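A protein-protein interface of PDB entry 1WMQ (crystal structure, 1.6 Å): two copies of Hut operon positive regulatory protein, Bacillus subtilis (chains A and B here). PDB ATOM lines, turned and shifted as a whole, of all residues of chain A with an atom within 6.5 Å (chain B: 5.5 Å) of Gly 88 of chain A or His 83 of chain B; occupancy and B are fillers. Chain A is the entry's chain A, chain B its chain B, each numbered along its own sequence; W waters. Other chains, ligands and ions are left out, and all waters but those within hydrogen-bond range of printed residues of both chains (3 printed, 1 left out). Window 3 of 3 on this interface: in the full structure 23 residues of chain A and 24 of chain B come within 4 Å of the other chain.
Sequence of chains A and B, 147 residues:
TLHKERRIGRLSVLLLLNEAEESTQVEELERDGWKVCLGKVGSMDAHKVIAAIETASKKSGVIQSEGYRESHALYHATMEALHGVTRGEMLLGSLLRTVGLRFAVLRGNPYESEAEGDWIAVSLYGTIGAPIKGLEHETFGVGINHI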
ATOM      1  N   GLU A  80      37.540  27.070  -6.782  1.00  0.00           N
ATOM      2  CA  GLU A  80      36.655  27.940  -6.018  1.00  0.00           C
ATOM      3  C   GLU A  80      35.583  28.572  -6.906  1.00  0.00           C
ATOM      4  O   GLU A  80      34.424  28.660  -6.507  1.00  0.00           O
ATOM      5  CB  GLU A  80      37.471  28.995  -5.249  1.00  0.00           C
ATOM      6  CG  GLU A  80      38.407  28.350  -4.209  1.00  0.00           C
ATOM      7  CD  GLU A  80      38.842  29.284  -3.085  1.00  0.00           C
ATOM      8  OE1 GLU A  80      38.725  30.513  -3.246  1.00  0.00           O
ATOM      9  N   LEU A  82      34.375  27.256  -9.556  1.00  0.00           N
ATOM     10  CA  LEU A  82      33.452  26.186  -9.910  1.00  0.00           C
ATOM     11  C   LEU A  82      32.412  25.913  -8.827  1.00  0.00           C
ATOM     12  O   LEU A  82      31.335  25.402  -9.124  1.00  0.00           O
ATOM     13  CB  LEU A  82      34.217  24.903 -10.246  1.00  0.00           C
ATOM     14  CG  LEU A  82      34.805  24.939 -11.653  1.00  0.00           C
ATOM     15  CD1 LEU A  82      35.721  23.741 -11.853  1.00  0.00           C
ATOM     16  CD2 LEU A  82      33.676  24.946 -12.680  1.00  0.00           C
ATOM     17  N   HIS A  83      32.710  26.268  -7.581  1.00  0.00           N
ATOM     18  CA  HIS A  83      31.731  26.040  -6.515  1.00  0.00           C
ATOM     19  C   HIS A  83      30.485  26.888  -6.750  1.00  0.00           C
ATOM     20  O   HIS A  83      29.358  26.446  -6.495  1.00  0.00           O
ATOM     21  CB  HIS A  83      32.323  26.382  -5.141  1.00  0.00           C
ATOM     22  CG  HIS A  83      32.964  25.217  -4.460  1.00  0.00           C
ATOM     23  ND1 HIS A  83      34.328  25.023  -4.439  1.00  0.00           N
ATOM     24  CD2 HIS A  83      32.423  24.159  -3.812  1.00  0.00           C
ATOM     25  CE1 HIS A  83      34.600  23.895  -3.808  1.00  0.00           C
ATOM     26  NE2 HIS A  83      33.462  23.350  -3.417  1.00  0.00           N
ATOM     27  N   GLY A  84      30.692  28.105  -7.240  1.00  0.00           N
ATOM     28  CA  GLY A  84      29.579  28.999  -7.488  1.00  0.00           C
ATOM     29  C   GLY A  84      28.748  28.505  -8.650  1.00  0.00           C
ATOM     30  O   GLY A  84      27.532  28.672  -8.681  1.00  0.00           O
ATOM     31  N   THR A  86      28.582  25.155  -9.766  1.00  0.00           N
ATOM     32  CA  THR A  86      27.959  23.864  -9.475  1.00  0.00           C
ATOM     33  C   THR A  86      27.111  23.789  -8.212  1.00  0.00           C
ATOM     34  O   THR A  86      26.240  22.930  -8.106  1.00  0.00           O
ATOM     35  CB  THR A  86      29.009  22.741  -9.432  1.00  0.00           C
ATOM     36  OG1 THR A  86      30.022  23.061  -8.475  1.00  0.00           O
ATOM     37  CG2 THR A  86      29.645  22.571 -10.816  1.00  0.00           C
ATOM     38  N   ARG A  87      27.390  24.669  -7.259  1.00  0.00           N
ATOM     39  CA  ARG A  87      26.616  24.748  -6.021  1.00  0.00           C
ATOM     40  C   ARG A  87      26.345  23.452  -5.240  1.00  0.00           C
ATOM     41  O   ARG A  87      25.193  23.105  -4.984  1.00  0.00           O
ATOM     42  CB  ARG A  87      25.292  25.470  -6.311  1.00  0.00           C
ATOM     43  CG  ARG A  87      25.448  26.955  -6.623  1.00  0.00           C
ATOM     44  CD  ARG A  87      24.423  27.431  -7.644  1.00  0.00           C
ATOM     45  NE  ARG A  87      24.659  26.775  -8.932  1.00  0.00           N
ATOM     46  CZ  ARG A  87      23.768  26.032  -9.581  1.00  0.00           C
ATOM     47  NH1 ARG A  87      22.552  25.840  -9.086  1.00  0.00           N
ATOM     48  NH2 ARG A  87      24.119  25.437 -10.715  1.00  0.00           N
ATOM     49  N   GLY A  88      27.394  22.736  -4.854  1.00  0.00           N
ATOM     50  CA  GLY A  88      27.176  21.533  -4.063  1.00  0.00           C
ATOM     51  C   GLY A  88      27.864  20.280  -4.542  1.00  0.00           C
ATOM     52  O   GLY A  88      28.510  19.576  -3.771  1.00  0.00           O
ATOM     53  N   GLU A  89      27.711  19.990  -5.825  1.00  0.00           N
ATOM     54  CA  GLU A  89      28.331  18.810  -6.401  1.00  0.00           C
ATOM     55  C   GLU A  89      29.096  19.315  -7.613  1.00  0.00           C
ATOM     56  O   GLU A  89      28.485  19.838  -8.545  1.00  0.00           O
ATOM     57  CB  GLU A  89      27.259  17.811  -6.843  1.00  0.00           C
ATOM     58  CG  GLU A  89      26.112  17.598  -5.854  1.00  0.00           C
ATOM     59  CD  GLU A  89      26.575  17.361  -4.430  1.00  0.00           C
ATOM     60  OE1 GLU A  89      27.532  16.587  -4.224  1.00  0.00           O
ATOM     61  OE2 GLU A  89      25.966  17.946  -3.506  1.00  0.00           O
ATOM     62  N   MET A  90      30.420  19.171  -7.602  1.00  0.00           N
ATOM     63  CA  MET A  90      31.229  19.658  -8.717  1.00  0.00           C
ATOM     64  C   MET A  90      31.161  18.653  -9.855  1.00  0.00           C
ATOM     65  O   MET A  90      32.176  18.096 -10.291  1.00  0.00           O
ATOM     66  CB  MET A  90      32.680  19.881  -8.281  1.00  0.00           C
ATOM     67  CG  MET A  90      33.422  20.872  -9.169  1.00  0.00           C
ATOM     68  SD  MET A  90      34.959  21.445  -8.444  1.00  0.00           S
ATOM     69  CE  MET A  90      34.329  22.496  -7.137  1.00  0.00           C
ATOM     70  N   LEU A  91      29.938  18.453 -10.333  1.00  0.00           N
ATOM     71  CA  LEU A  91      29.630  17.498 -11.386  1.00  0.00           C
ATOM     72  C   LEU A  91      28.717  18.114 -12.428  1.00  0.00           C
ATOM     73  O   LEU A  91      27.809  18.877 -12.104  1.00  0.00           O
ATOM     74  CB  LEU A  91      28.926  16.291 -10.772  1.00  0.00           C
ATOM     75  CG  LEU A  91      29.688  15.609  -9.638  1.00  0.00           C
ATOM     76  CD1 LEU A  91      28.779  14.619  -8.904  1.00  0.00           C
ATOM     77  CD2 LEU A  91      30.898  14.903 -10.220  1.00  0.00           C
ATOM     78  N   ARG A  97      23.672  17.445 -16.527  1.00  0.00           N
ATOM     79  CA  ARG A  97      23.624  18.875 -16.772  1.00  0.00           C
ATOM     80  C   ARG A  97      24.839  19.321 -17.572  1.00  0.00           C
ATOM     81  O   ARG A  97      25.897  18.675 -17.571  1.00  0.00           O
ATOM     82  CB  ARG A  97      23.472  19.680 -15.469  1.00  0.00           C
ATOM     83  CG  ARG A  97      24.584  19.553 -14.463  1.00  0.00           C
ATOM     84  CD  ARG A  97      24.293  20.451 -13.244  1.00  0.00           C
ATOM     85  NE  ARG A  97      25.324  20.283 -12.228  1.00  0.00           N
ATOM     86  CZ  ARG A  97      25.316  20.866 -11.034  1.00  0.00           C
ATOM     87  NH1 ARG A  97      24.325  21.677 -10.680  1.00  0.00           N
ATOM     88  NH2 ARG A  97      26.304  20.613 -10.186  1.00  0.00           N
ATOM     89  N   THR B  78      18.911  31.565  -1.824  1.00  0.00           N
ATOM     90  CA  THR B  78      19.921  32.120  -0.947  1.00  0.00           C
ATOM     91  C   THR B  78      20.990  31.071  -0.655  1.00  0.00           C
ATOM     92  O   THR B  78      22.182  31.396  -0.618  1.00  0.00           O
ATOM     93  CB  THR B  78      19.300  32.609   0.369  1.00  0.00           C
ATOM     94  OG1 THR B  78      18.363  33.654   0.076  1.00  0.00           O
ATOM     95  CG2 THR B  78      20.376  33.143   1.309  1.00  0.00           C
ATOM     96  N   MET B  79      20.560  29.827  -0.447  1.00  0.00           N
ATOM     97  CA  MET B  79      21.496  28.735  -0.186  1.00  0.00           C
ATOM     98  C   MET B  79      22.451  28.606  -1.369  1.00  0.00           C
ATOM     99  O   MET B  79      23.665  28.462  -1.188  1.00  0.00           O
ATOM    100  CB  MET B  79      20.748  27.412  -0.013  1.00  0.00           C
ATOM    101  CG  MET B  79      19.984  27.275   1.291  1.00  0.00           C
ATOM    102  SD  MET B  79      21.043  27.308   2.738  1.00  0.00           S
ATOM    103  N   GLU B  80      21.901  28.657  -2.577  1.00  0.00           N
ATOM    104  CA  GLU B  80      22.744  28.535  -3.759  1.00  0.00           C
ATOM    105  C   GLU B  80      23.737  29.690  -3.883  1.00  0.00           C
ATOM    106  O   GLU B  80      24.890  29.474  -4.251  1.00  0.00           O
ATOM    107  CB  GLU B  80      21.872  28.377  -5.014  1.00  0.00           C
ATOM    108  CG  GLU B  80      21.210  26.990  -5.050  1.00  0.00           C
ATOM    109  CD  GLU B  80      20.543  26.642  -6.373  1.00  0.00           C
ATOM    110  OE1 GLU B  80      20.802  27.328  -7.377  1.00  0.00           O
ATOM    111  OE2 GLU B  80      19.763  25.667  -6.404  1.00  0.00           O
ATOM    112  N   ALA B  81      23.313  30.909  -3.558  1.00  0.00           N
ATOM    113  CA  ALA B  81      24.227  32.042  -3.628  1.00  0.00           C
ATOM    114  C   ALA B  81      25.318  31.869  -2.572  1.00  0.00           C
ATOM    115  O   ALA B  81      26.479  32.224  -2.801  1.00  0.00           O
ATOM    116  CB  ALA B  81      23.465  33.355  -3.396  1.00  0.00           C
ATOM    117  N   LEU B  82      24.957  31.331  -1.408  1.00  0.00           N
ATOM    118  CA  LEU B  82      25.954  31.142  -0.366  1.00  0.00           C
ATOM    119  C   LEU B  82      27.046  30.148  -0.756  1.00  0.00           C
ATOM    120  O   LEU B  82      28.153  30.214  -0.225  1.00  0.00           O
ATOM    121  CB  LEU B  82      25.293  30.716   0.946  1.00  0.00           C
ATOM    122  CG  LEU B  82      24.617  31.867   1.688  1.00  0.00           C
ATOM    123  CD1 LEU B  82      23.792  31.329   2.853  1.00  0.00           C
ATOM    124  CD2 LEU B  82      25.682  32.835   2.185  1.00  0.00           C
ATOM    125  N   HIS B  83      26.751  29.236  -1.678  1.00  0.00           N
ATOM    126  CA  HIS B  83      27.780  28.283  -2.112  1.00  0.00           C
ATOM    127  C   HIS B  83      28.935  29.032  -2.761  1.00  0.00           C
ATOM    128  O   HIS B  83      30.099  28.668  -2.590  1.00  0.00           O
ATOM    129  CB  HIS B  83      27.194  27.286  -3.120  1.00  0.00           C
ATOM    130  CG  HIS B  83      26.621  26.058  -2.486  1.00  0.00           C
ATOM    131  ND1 HIS B  83      27.405  25.075  -1.919  1.00  0.00           N
ATOM    132  CD2 HIS B  83      25.336  25.662  -2.308  1.00  0.00           C
ATOM    133  CE1 HIS B  83      26.630  24.127  -1.422  1.00  0.00           C
ATOM    134  NE2 HIS B  83      25.370  24.460  -1.647  1.00  0.00           N
ATOM    135  N   GLY B  84      28.603  30.072  -3.517  1.00  0.00           N
ATOM    136  CA  GLY B  84      29.628  30.839  -4.193  1.00  0.00           C
ATOM    137  C   GLY B  84      30.462  31.613  -3.203  1.00  0.00           C
ATOM    138  O   GLY B  84      31.665  31.803  -3.394  1.00  0.00           O
ATOM    139  N   VAL B  85      29.816  32.055  -2.131  1.00  0.00           N
ATOM    140  CA  VAL B  85      30.496  32.819  -1.110  1.00  0.00           C
ATOM    141  C   VAL B  85      31.357  31.957  -0.193  1.00  0.00           C
ATOM    142  O   VAL B  85      32.482  32.333   0.118  1.00  0.00           O
ATOM    143  CB  VAL B  85      29.481  33.600  -0.237  1.00  0.00           C
ATOM    144  CG1 VAL B  85      30.175  34.191   0.975  1.00  0.00           C
ATOM    145  CG2 VAL B  85      28.830  34.710  -1.061  1.00  0.00           C
ATOM    146  N   THR B  86      30.839  30.796   0.211  1.00  0.00           N
ATOM    147  CA  THR B  86      31.561  29.924   1.134  1.00  0.00           C
ATOM    148  C   THR B  86      32.470  28.882   0.499  1.00  0.00           C
ATOM    149  O   THR B  86      33.409  28.407   1.141  1.00  0.00           O
ATOM    150  CB  THR B  86      30.608  29.239   2.115  1.00  0.00           C
ATOM    151  OG1 THR B  86      29.608  28.520   1.393  1.00  0.00           O
ATOM    152  CG2 THR B  86      29.939  30.291   3.015  1.00  0.00           C
ATOM    153  N   ARG B  87      32.167  28.507  -0.738  1.00  0.00           N
ATOM    154  CA  ARG B  87      33.003  27.569  -1.484  1.00  0.00           C
ATOM    155  C   ARG B  87      33.393  26.244  -0.816  1.00  0.00           C
ATOM    156  O   ARG B  87      34.580  25.943  -0.670  1.00  0.00           O
ATOM    157  CB  ARG B  87      34.263  28.301  -1.962  1.00  0.00           C
ATOM    158  CG  ARG B  87      33.999  29.324  -3.065  1.00  0.00           C
ATOM    159  CD  ARG B  87      34.922  30.538  -2.970  1.00  0.00           C
ATOM    160  NE  ARG B  87      34.680  31.254  -1.716  1.00  0.00           N
ATOM    161  CZ  ARG B  87      35.603  31.482  -0.787  1.00  0.00           C
ATOM    162  NH1 ARG B  87      36.851  31.062  -0.961  1.00  0.00           N
ATOM    163  NH2 ARG B  87      35.268  32.107   0.335  1.00  0.00           N
ATOM    164  N   GLY B  88      32.408  25.442  -0.418  1.00  0.00           N
ATOM    165  CA  GLY B  88      32.723  24.148   0.173  1.00  0.00           C
ATOM    166  C   GLY B  88      32.115  23.862   1.523  1.00  0.00           C
ATOM    167  O   GLY B  88      31.544  22.798   1.755  1.00  0.00           O
ATOM    168  N   MET B  90      29.562  25.712   4.230  1.00  0.00           N
ATOM    169  CA  MET B  90      28.663  26.838   4.459  1.00  0.00           C
ATOM    170  C   MET B  90      28.752  27.266   5.914  1.00  0.00           C
ATOM    171  O   MET B  90      27.761  27.273   6.655  1.00  0.00           O
ATOM    172  CB  MET B  90      27.223  26.466   4.091  1.00  0.00           C
ATOM    173  CG  MET B  90      26.395  27.669   3.640  1.00  0.00           C
ATOM    174  SD  MET B  90      24.821  27.209   2.885  1.00  0.00           S
ATOM    175  CE  MET B  90      25.373  26.668   1.251  1.00  0.00           C
HETATM  176  O   HOH W   1      21.542  29.022  -8.945  1.00  0.00           O
HETATM  177  O   HOH W   2      32.561  30.546  -6.089  1.00  0.00           O
HETATM  178  O   HOH W   3      26.669  30.324  -6.087  1.00  0.00           O
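Water W1 lies within hydrogen-bond range of the side-chain carboxylate of Glu 80 of chain B (2.4 Å) and the guanidinium group of Arg 87 of chain A (3.3 Å). Water W2 lies within hydrogen-bond range of O of Glu 80 of chain A (2.7 Å), O of Gly 84 of chain B (3.1 Å) and N of Gly 84 of chain A (3.3 Å). Water W3 lies within hydrogen-bond range of the backbone carbonyl oxygen (O) of Glu 80 of chain B, the backbone carbonyl oxygen (O) of Gly 84 of chain A and the backbone NH (N) of Gly 84 of chain B.
Among the printed residues, merely in contact across the chains: Arg 87 of chain A with His 83 of chain B, His 83 of chain A with Gly 88 of chain B, Gly 88 of chain A with His 83 of chain B, His 83 of chain A with Arg 87 of chain B and Gly 84 of chain A with Gly 84 of chain B.
Along chain B the printed residues that touch a printed residue of chain A span positions 80 to 88. Among the printed residues, 7 pairs touch across the chains. Among the printed residues, Asp or Glu carboxylates within 4 Å of a Lys or Arg side-chain nitrogen of the other chain: Glu 80 of chain A with Arg 87 of chain B and Arg 87 of chain A with Glu 80 of chain B.
Glu 80 of chain A touches Arg 87 of chain B, and with the chains exchanged Arg 87 of chain A touches Glu 80 of chain B. His 83 of chain A touches Arg 87 of chain B, and with the chains exchanged Arg 87 of chain A touches His 83 of chain B. His 83 of chain A touches Gly 88 of chain B, and with the chains exchanged Gly 88 of chain A touches His 83 of chain B. Gly 84 of chain B touches its own counterpart, Gly 84 of chain A. Positions printed for both chains: 80, 82, 83, 84, 86, 87, 88 and 90. Of the 7 pairs that touch across the chains among the printed residues, 7 have their exchanged pair printed and touching as well.
OE1 of Glu 80 of chain A lies within salt-bridge range of NH1 of Arg 87 of chain B (3.0 Å). OE1 of Glu 80 of chain B is in salt-bridge range of NH1 of Arg 87 of chain A.
Of the printed residues of chain B, Glu 80 of chain A touches Arg 87. Of the printed residues of chain B, His 83 of chain A touches Arg 87 and Gly 88. Of the printed residues of chain B, Gly 84 of chain A touches Gly 84 (3.8 Å). Of chain B, only His 83 comes within 4 Å of Gly 88 of chain A. Glu 89 of chain A touches none of the printed residues of chain B. Of the printed residues of chain A, Glu 80 of chain B touches Arg 87. Of chain A, only Arg 87 and Gly 88 come within 4 Å of His 83 of chain B. The nearest printed residue of chain B that does not touch Gly 88 of chain A is Gly 88 of chain B (7.1 Å). The nearest residue of chain A that does not touch His 83 of chain B is His 83 of chain A (4.1 Å).
O of Gly 84 of chain A sits close to NE of Arg 87 of chain A (3.5 Å). The guanidinium group of Arg 87 of chain B lies close to the backbone carbonyl oxygen of Gly 84 of chain B. The backbone carbonyl oxygen of Val 85 of chain B sits at hydrogen-bond distance from the guanidinium group of Arg 87 of chain B, 2.8 Å away.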
